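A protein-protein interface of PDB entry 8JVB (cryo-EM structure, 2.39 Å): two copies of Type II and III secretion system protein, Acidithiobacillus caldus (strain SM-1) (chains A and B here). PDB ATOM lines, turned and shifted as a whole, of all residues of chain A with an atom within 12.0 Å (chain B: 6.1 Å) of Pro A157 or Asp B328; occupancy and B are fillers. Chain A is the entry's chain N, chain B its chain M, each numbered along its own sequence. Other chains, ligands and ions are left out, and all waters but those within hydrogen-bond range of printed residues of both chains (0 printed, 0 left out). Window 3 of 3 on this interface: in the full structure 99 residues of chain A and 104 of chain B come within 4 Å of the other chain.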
ATOM      1  N   GLY A 128      20.526  14.537  13.701  1.00  0.00           N
ATOM      2  CA  GLY A 128      19.391  14.808  14.559  1.00  0.00           C
ATOM      3  C   GLY A 128      18.509  13.586  14.680  1.00  0.00           C
ATOM      4  O   GLY A 128      18.527  12.720  13.801  1.00  0.00           O
ATOM      5  N   LYS A 129      17.726  13.497  15.751  1.00  0.00           N
ATOM      6  CA  LYS A 129      16.950  12.282  16.024  1.00  0.00           C
ATOM      7  C   LYS A 129      15.541  12.380  15.444  1.00  0.00           C
ATOM      8  O   LYS A 129      15.157  11.583  14.586  1.00  0.00           O
ATOM      9  CB  LYS A 129      16.911  12.013  17.529  1.00  0.00           C
ATOM     10  CG  LYS A 129      18.235  11.536  18.105  1.00  0.00           C
ATOM     11  CD  LYS A 129      18.042  10.537  19.242  1.00  0.00           C
ATOM     12  CE  LYS A 129      17.022   9.452  18.912  1.00  0.00           C
ATOM     13  NZ  LYS A 129      17.158   8.904  17.529  1.00  0.00           N
ATOM     14  N   ASN A 130      14.766  13.354  15.903  1.00  0.00           N
ATOM     15  CA  ASN A 130      13.365  13.497  15.516  1.00  0.00           C
ATOM     16  C   ASN A 130      13.152  14.892  14.943  1.00  0.00           C
ATOM     17  O   ASN A 130      12.790  15.826  15.663  1.00  0.00           O
ATOM     18  CB  ASN A 130      12.448  13.233  16.710  1.00  0.00           C
ATOM     19  CG  ASN A 130      12.550  11.812  17.220  1.00  0.00           C
ATOM     20  OD1 ASN A 130      11.820  10.928  16.775  1.00  0.00           O
ATOM     21  ND2 ASN A 130      13.460  11.585  18.158  1.00  0.00           N
ATOM     22  N   LEU A 131      13.372  15.032  13.642  1.00  0.00           N
ATOM     23  CA  LEU A 131      13.196  16.310  12.977  1.00  0.00           C
ATOM     24  C   LEU A 131      11.951  16.289  12.100  1.00  0.00           C
ATOM     25  O   LEU A 131      11.596  15.268  11.505  1.00  0.00           O
ATOM     26  CB  LEU A 131      14.425  16.657  12.139  1.00  0.00           C
ATOM     27  CG  LEU A 131      15.780  16.608  12.843  1.00  0.00           C
ATOM     28  CD1 LEU A 131      16.846  17.242  11.973  1.00  0.00           C
ATOM     29  CD2 LEU A 131      15.712  17.301  14.193  1.00  0.00           C
ATOM     30  N   ALA A 132      11.286  17.436  12.029  1.00  0.00           N
ATOM     31  CA  ALA A 132      10.081  17.559  11.230  1.00  0.00           C
ATOM     32  C   ALA A 132      10.411  17.456   9.743  1.00  0.00           C
ATOM     33  O   ALA A 132      11.522  17.790   9.322  1.00  0.00           O
ATOM     34  CB  ALA A 132       9.387  18.884  11.514  1.00  0.00           C
ATOM     35  N   PRO A 133       9.462  16.979   8.930  1.00  0.00           N
ATOM     36  CA  PRO A 133       9.693  16.896   7.482  1.00  0.00           C
ATOM     37  C   PRO A 133      10.092  18.229   6.873  1.00  0.00           C
ATOM     38  O   PRO A 133      10.893  18.277   5.934  1.00  0.00           O
ATOM     39  CB  PRO A 133       8.339  16.425   6.940  1.00  0.00           C
ATOM     40  CG  PRO A 133       7.728  15.664   8.054  1.00  0.00           C
ATOM     41  CD  PRO A 133       8.292  16.190   9.350  1.00  0.00           C
ATOM     42  N   THR A 134       9.527  19.318   7.396  1.00  0.00           N
ATOM     43  CA  THR A 134       9.891  20.648   6.927  1.00  0.00           C
ATOM     44  C   THR A 134      11.373  20.918   7.152  1.00  0.00           C
ATOM     45  O   THR A 134      12.063  21.463   6.284  1.00  0.00           O
ATOM     46  CB  THR A 134       9.039  21.703   7.634  1.00  0.00           C
ATOM     47  OG1 THR A 134       8.836  21.317   8.998  1.00  0.00           O
ATOM     48  CG2 THR A 134       7.691  21.843   6.947  1.00  0.00           C
ATOM     49  N   LEU A 136      13.808  18.662   7.463  1.00  0.00           N
ATOM     50  CA  LEU A 136      14.575  17.848   6.524  1.00  0.00           C
ATOM     51  C   LEU A 136      14.527  18.430   5.119  1.00  0.00           C
ATOM     52  O   LEU A 136      15.551  18.486   4.427  1.00  0.00           O
ATOM     53  CB  LEU A 136      14.064  16.409   6.522  1.00  0.00           C
ATOM     54  CG  LEU A 136      14.888  15.388   7.306  1.00  0.00           C
ATOM     55  CD1 LEU A 136      15.099  15.837   8.738  1.00  0.00           C
ATOM     56  CD2 LEU A 136      14.228  14.022   7.260  1.00  0.00           C
ATOM     57  N   ALA A 153      20.869  13.124   9.935  1.00  0.00           N
ATOM     58  CA  ALA A 153      19.630  13.350  10.661  1.00  0.00           C
ATOM     59  C   ALA A 153      18.516  12.471  10.104  1.00  0.00           C
ATOM     60  O   ALA A 153      18.493  12.129   8.919  1.00  0.00           O
ATOM     61  CB  ALA A 153      19.227  14.820  10.581  1.00  0.00           C
ATOM     62  N   THR A 154      17.582  12.110  10.977  1.00  0.00           N
ATOM     63  CA  THR A 154      16.480  11.234  10.618  1.00  0.00           C
ATOM     64  C   THR A 154      15.158  11.881  10.996  1.00  0.00           C
ATOM     65  O   THR A 154      15.098  12.681  11.933  1.00  0.00           O
ATOM     66  CB  THR A 154      16.605   9.874  11.319  1.00  0.00           C
ATOM     67  OG1 THR A 154      17.249  10.046  12.587  1.00  0.00           O
ATOM     68  CG2 THR A 154      17.416   8.911  10.471  1.00  0.00           C
ATOM     69  N   PRO A 155      14.085  11.559  10.280  1.00  0.00           N
ATOM     70  CA  PRO A 155      12.778  12.132  10.601  1.00  0.00           C
ATOM     71  C   PRO A 155      12.100  11.383  11.742  1.00  0.00           C
ATOM     72  O   PRO A 155      12.517  10.302  12.156  1.00  0.00           O
ATOM     73  CB  PRO A 155      11.999  11.967   9.294  1.00  0.00           C
ATOM     74  CG  PRO A 155      12.577  10.739   8.693  1.00  0.00           C
ATOM     75  CD  PRO A 155      14.040  10.742   9.055  1.00  0.00           C
ATOM     76  N   SER A 156      11.035  11.991  12.246  1.00  0.00           N
ATOM     77  CA  SER A 156      10.198  11.362  13.250  1.00  0.00           C
ATOM     78  C   SER A 156       9.309  10.305  12.605  1.00  0.00           C
ATOM     79  O   SER A 156       9.048  10.352  11.402  1.00  0.00           O
ATOM     80  CB  SER A 156       9.346  12.415  13.952  1.00  0.00           C
ATOM     81  OG  SER A 156      10.136  13.506  14.379  1.00  0.00           O
ATOM     82  N   PRO A 157       8.844   9.323  13.383  1.00  0.00           N
ATOM     83  CA  PRO A 157       7.915   8.333  12.812  1.00  0.00           C
ATOM     84  C   PRO A 157       6.651   8.959  12.255  1.00  0.00           C
ATOM     85  O   PRO A 157       6.134   8.502  11.229  1.00  0.00           O
ATOM     86  CB  PRO A 157       7.616   7.408  14.001  1.00  0.00           C
ATOM     87  CG  PRO A 157       8.737   7.618  14.951  1.00  0.00           C
ATOM     88  CD  PRO A 157       9.163   9.038  14.792  1.00  0.00           C
ATOM     89  N   PHE A 158       6.141   9.998  12.908  1.00  0.00           N
ATOM     90  CA  PHE A 158       4.967  10.717  12.440  1.00  0.00           C
ATOM     91  C   PHE A 158       4.969  12.091  13.091  1.00  0.00           C
ATOM     92  O   PHE A 158       5.717  12.352  14.034  1.00  0.00           O
ATOM     93  CB  PHE A 158       3.675   9.953  12.750  1.00  0.00           C
ATOM     94  CG  PHE A 158       3.453   9.694  14.214  1.00  0.00           C
ATOM     95  CD1 PHE A 158       2.817  10.630  15.012  1.00  0.00           C
ATOM     96  CD2 PHE A 158       3.874   8.510  14.792  1.00  0.00           C
ATOM     97  CE1 PHE A 158       2.614  10.395  16.354  1.00  0.00           C
ATOM     98  CE2 PHE A 158       3.672   8.268  16.133  1.00  0.00           C
ATOM     99  CZ  PHE A 158       3.041   9.211  16.915  1.00  0.00           C
ATOM    100  N   ASP A 159       4.120  12.969  12.572  1.00  0.00           N
ATOM    101  CA  ASP A 159       3.960  14.314  13.106  1.00  0.00           C
ATOM    102  C   ASP A 159       2.682  14.383  13.926  1.00  0.00           C
ATOM    103  O   ASP A 159       1.630  13.916  13.482  1.00  0.00           O
ATOM    104  CB  ASP A 159       3.918  15.349  11.984  1.00  0.00           C
ATOM    105  CG  ASP A 159       5.214  15.419  11.212  1.00  0.00           C
ATOM    106  OD1 ASP A 159       6.208  15.926  11.770  1.00  0.00           O
ATOM    107  OD2 ASP A 159       5.239  14.970  10.048  1.00  0.00           O
ATOM    108  N   MET A 160       2.776  14.961  15.120  1.00  0.00           N
ATOM    109  CA  MET A 160       1.601  15.137  15.964  1.00  0.00           C
ATOM    110  C   MET A 160       0.735  16.245  15.384  1.00  0.00           C
ATOM    111  O   MET A 160       1.104  17.422  15.429  1.00  0.00           O
ATOM    112  CB  MET A 160       2.015  15.459  17.396  1.00  0.00           C
ATOM    113  CG  MET A 160       2.172  14.239  18.289  1.00  0.00           C
ATOM    114  SD  MET A 160       0.623  13.368  18.587  1.00  0.00           S
ATOM    115  CE  MET A 160       0.031  14.205  20.052  1.00  0.00           C
ATOM    116  N   GLU A 161      -0.414  15.872  14.831  1.00  0.00           N
ATOM    117  CA  GLU A 161      -1.344  16.843  14.286  1.00  0.00           C
ATOM    118  C   GLU A 161      -2.190  17.457  15.396  1.00  0.00           C
ATOM    119  O   GLU A 161      -2.119  17.067  16.563  1.00  0.00           O
ATOM    120  CB  GLU A 161      -2.243  16.194  13.235  1.00  0.00           C
ATOM    121  CG  GLU A 161      -1.506  15.512  12.097  1.00  0.00           C
ATOM    122  CD  GLU A 161      -0.882  16.484  11.108  1.00  0.00           C
ATOM    123  OE1 GLU A 161      -0.797  17.693  11.403  1.00  0.00           O
ATOM    124  OE2 GLU A 161      -0.484  16.033  10.015  1.00  0.00           O
ATOM    125  N   LYS A 162      -2.999  18.437  15.016  1.00  0.00           N
ATOM    126  CA  LYS A 162      -3.929  19.066  15.936  1.00  0.00           C
ATOM    127  C   LYS A 162      -5.268  18.344  15.887  1.00  0.00           C
ATOM    128  O   LYS A 162      -5.688  17.861  14.834  1.00  0.00           O
ATOM    129  CB  LYS A 162      -4.111  20.544  15.594  1.00  0.00           C
ATOM    130  CG  LYS A 162      -2.981  21.426  16.083  1.00  0.00           C
ATOM    131  CD  LYS A 162      -3.280  22.891  15.848  1.00  0.00           C
ATOM    132  CE  LYS A 162      -2.182  23.547  15.037  1.00  0.00           C
ATOM    133  NZ  LYS A 162      -2.107  25.011  15.280  1.00  0.00           N
ATOM    134  N   ARG A 283      -8.326  14.216  13.922  1.00  0.00           N
ATOM    135  CA  ARG A 283      -7.073  14.942  13.796  1.00  0.00           C
ATOM    136  C   ARG A 283      -6.977  15.599  12.422  1.00  0.00           C
ATOM    137  O   ARG A 283      -7.606  15.169  11.454  1.00  0.00           O
ATOM    138  CB  ARG A 283      -5.882  14.010  14.022  1.00  0.00           C
ATOM    139  CG  ARG A 283      -5.719  12.929  12.973  1.00  0.00           C
ATOM    140  CD  ARG A 283      -4.388  12.220  13.119  1.00  0.00           C
ATOM    141  NE  ARG A 283      -4.086  11.382  11.966  1.00  0.00           N
ATOM    142  CZ  ARG A 283      -3.988  10.060  12.003  1.00  0.00           C
ATOM    143  NH1 ARG A 283      -4.154   9.384  13.126  1.00  0.00           N
ATOM    144  NH2 ARG A 283      -3.716   9.400  10.881  1.00  0.00           N
ATOM    145  N   LYS B 162       7.108  -1.232  20.766  1.00  0.00           N
ATOM    146  CA  LYS B 162       6.421  -0.947  22.013  1.00  0.00           C
ATOM    147  C   LYS B 162       4.997  -1.483  21.948  1.00  0.00           C
ATOM    148  O   LYS B 162       4.365  -1.476  20.890  1.00  0.00           O
ATOM    149  CB  LYS B 162       6.409   0.555  22.291  1.00  0.00           C
ATOM    150  CG  LYS B 162       7.714   1.082  22.854  1.00  0.00           C
ATOM    151  CD  LYS B 162       7.601   2.538  23.245  1.00  0.00           C
ATOM    152  CE  LYS B 162       8.655   3.374  22.549  1.00  0.00           C
ATOM    153  NZ  LYS B 162       8.976   4.612  23.305  1.00  0.00           N
ATOM    154  N   ARG B 326       0.559   3.579  16.583  1.00  0.00           N
ATOM    155  CA  ARG B 326       1.918   4.008  16.275  1.00  0.00           C
ATOM    156  C   ARG B 326       2.400   4.885  17.422  1.00  0.00           C
ATOM    157  O   ARG B 326       1.654   5.735  17.906  1.00  0.00           O
ATOM    158  CB  ARG B 326       1.987   4.777  14.953  1.00  0.00           C
ATOM    159  CG  ARG B 326       2.193   3.903  13.734  1.00  0.00           C
ATOM    160  CD  ARG B 326       1.417   4.432  12.546  1.00  0.00           C
ATOM    161  NE  ARG B 326       2.256   5.239  11.668  1.00  0.00           N
ATOM    162  CZ  ARG B 326       1.934   6.449  11.230  1.00  0.00           C
ATOM    163  NH1 ARG B 326       0.794   7.027  11.567  1.00  0.00           N
ATOM    164  NH2 ARG B 326       2.781   7.095  10.436  1.00  0.00           N
ATOM    165  N   VAL B 327       3.644   4.684  17.847  1.00  0.00           N
ATOM    166  CA  VAL B 327       4.163   5.292  19.067  1.00  0.00           C
ATOM    167  C   VAL B 327       5.397   6.120  18.740  1.00  0.00           C
ATOM    168  O   VAL B 327       6.200   5.746  17.881  1.00  0.00           O
ATOM    169  CB  VAL B 327       4.488   4.227  20.133  1.00  0.00           C
ATOM    170  CG1 VAL B 327       4.892   4.880  21.444  1.00  0.00           C
ATOM    171  CG2 VAL B 327       3.298   3.322  20.344  1.00  0.00           C
ATOM    172  N   ASP B 328       5.538   7.250  19.431  1.00  0.00           N
ATOM    173  CA  ASP B 328       6.666   8.154  19.286  1.00  0.00           C
ATOM    174  C   ASP B 328       7.662   7.945  20.425  1.00  0.00           C
ATOM    175  O   ASP B 328       7.499   7.075  21.282  1.00  0.00           O
ATOM    176  CB  ASP B 328       6.183   9.605  19.252  1.00  0.00           C
ATOM    177  CG  ASP B 328       6.242  10.203  17.868  1.00  0.00           C
ATOM    178  OD1 ASP B 328       6.670   9.495  16.932  1.00  0.00           O
ATOM    179  OD2 ASP B 328       5.859  11.383  17.711  1.00  0.00           O
ATOM    180  N   ASP B 329       8.710   8.772  20.434  1.00  0.00           N
ATOM    181  CA  ASP B 329       9.707   8.702  21.496  1.00  0.00           C
ATOM    182  C   ASP B 329       9.193   9.263  22.815  1.00  0.00           C
ATOM    183  O   ASP B 329       9.737   8.926  23.872  1.00  0.00           O
ATOM    184  CB  ASP B 329      10.975   9.443  21.078  1.00  0.00           C
ATOM    185  CG  ASP B 329      11.980   8.539  20.400  1.00  0.00           C
ATOM    186  OD1 ASP B 329      11.672   7.347  20.204  1.00  0.00           O
ATOM    187  OD2 ASP B 329      13.084   9.018  20.067  1.00  0.00           O
ATOM    188  N   ASP B 330       8.167  10.110  22.782  1.00  0.00           N
ATOM    189  CA  ASP B 330       7.543  10.643  23.982  1.00  0.00           C
ATOM    190  C   ASP B 330       6.299   9.864  24.378  1.00  0.00           C
ATOM    191  O   ASP B 330       5.525  10.335  25.218  1.00  0.00           O
ATOM    192  CB  ASP B 330       7.192  12.118  23.792  1.00  0.00           C
ATOM    193  CG  ASP B 330       8.374  12.942  23.334  1.00  0.00           C
ATOM    194  OD1 ASP B 330       9.167  13.374  24.195  1.00  0.00           O
ATOM    195  OD2 ASP B 330       8.511  13.158  22.112  1.00  0.00           O
ATOM    196  N   ASN B 331       6.089   8.692  23.781  1.00  0.00           N
ATOM    197  CA  ASN B 331       4.924   7.845  24.031  1.00  0.00           C
ATOM    198  C   ASN B 331       3.625   8.515  23.596  1.00  0.00           C
ATOM    199  O   ASN B 331       2.562   8.255  24.159  1.00  0.00           O
ATOM    200  CB  ASN B 331       4.841   7.419  25.501  1.00  0.00           C
ATOM    201  CG  ASN B 331       5.977   6.501  25.906  1.00  0.00           C
ATOM    202  OD1 ASN B 331       6.714   5.998  25.063  1.00  0.00           O
ATOM    203  ND2 ASN B 331       6.119   6.278  27.203  1.00  0.00           N
ATOM    204  N   ASN B 332       3.697   9.381  22.589  1.00  0.00           N
ATOM    205  CA  ASN B 332       2.498   9.838  21.904  1.00  0.00           C
ATOM    206  C   ASN B 332       2.006   8.739  20.975  1.00  0.00           C
ATOM    207  O   ASN B 332       2.803   8.060  20.325  1.00  0.00           O
ATOM    208  CB  ASN B 332       2.778  11.113  21.111  1.00  0.00           C
ATOM    209  CG  ASN B 332       3.124  12.289  21.997  1.00  0.00           C
ATOM    210  OD1 ASN B 332       2.572  12.444  23.084  1.00  0.00           O
ATOM    211  ND2 ASN B 332       4.047  13.123  21.539  1.00  0.00           N
ATOM    212  N   VAL B 333       0.692   8.561  20.913  1.00  0.00           N
ATOM    213  CA  VAL B 333       0.092   7.466  20.161  1.00  0.00           C
ATOM    214  C   VAL B 333      -0.746   8.046  19.033  1.00  0.00           C
ATOM    215  O   VAL B 333      -1.697   8.796  19.281  1.00  0.00           O
ATOM    216  CB  VAL B 333      -0.758   6.554  21.059  1.00  0.00           C
ATOM    217  CG1 VAL B 333      -1.249   5.353  20.274  1.00  0.00           C
ATOM    218  CG2 VAL B 333       0.042   6.110  22.268  1.00  0.00           C
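1 position is printed for both chains. Of the 8 pairs that touch across the chains among the printed residues, none has its exchanged pair printed and touching as well.
Printed residues of chain B within 4 Å of Asn A130: Asp B329. Thr A134 touches none of the printed residues of chain B. Leu A136 touches none of the printed residues of chain B. Of the printed residues of chain B, Phe A158 touches Arg B326 (3.7 Å), Val B327 (3.8 Å), Asp B328 (3.3 Å) and Asn B332 (3.6 Å). Printed residues of chain B within 4 Å of Met A160: Asn B332. Arg B326 touches just these residues of chain A: Pro A157 and Phe A158. Val B327 touches just one residue of chain A: Phe A158 (3.8 Å). Asp B328 touches two residues of chain A. No residue of chain A comes within 4 Å of Asn B331. Asn B332 touches just these residues of chain A: Phe A158 and Met A160. No residue of chain A comes within 4 Å of Val B333. The nearest residue of chain B that does not touch Pro A157 is Val B327 (4.3 Å). The nearest residue of chain A that does not touch Asp B328 is Met A160 (4.7 Å).
Hydrophobic or aromatic side chains of chain A that line the printed part of chain B: Pro A157, Phe A158 and Met A160. Among the printed residues, 8 pairs touch across the chains. Among the printed residues, no Asp or Glu carboxylate lies within 4 Å of a Lys or Arg side-chain nitrogen of the other chain.
Among the printed residues, merely in contact across the chains: Pro A157 with Asp B328 (3.3 Å), Phe A158 with Asp B328 (3.3 Å), Phe A158 with Asn B332 (3.6 Å), Phe A158 with Arg B326 (3.7 Å), Pro A157 with Arg B326 (3.7 Å), Phe A158 with Val B327 (3.8 Å) and Met A160 with Asn B332 (3.9 Å).
OD2 of Asp B329 is in hydrogen-bond range of ND2 of Asn A130 (3.2 Å).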
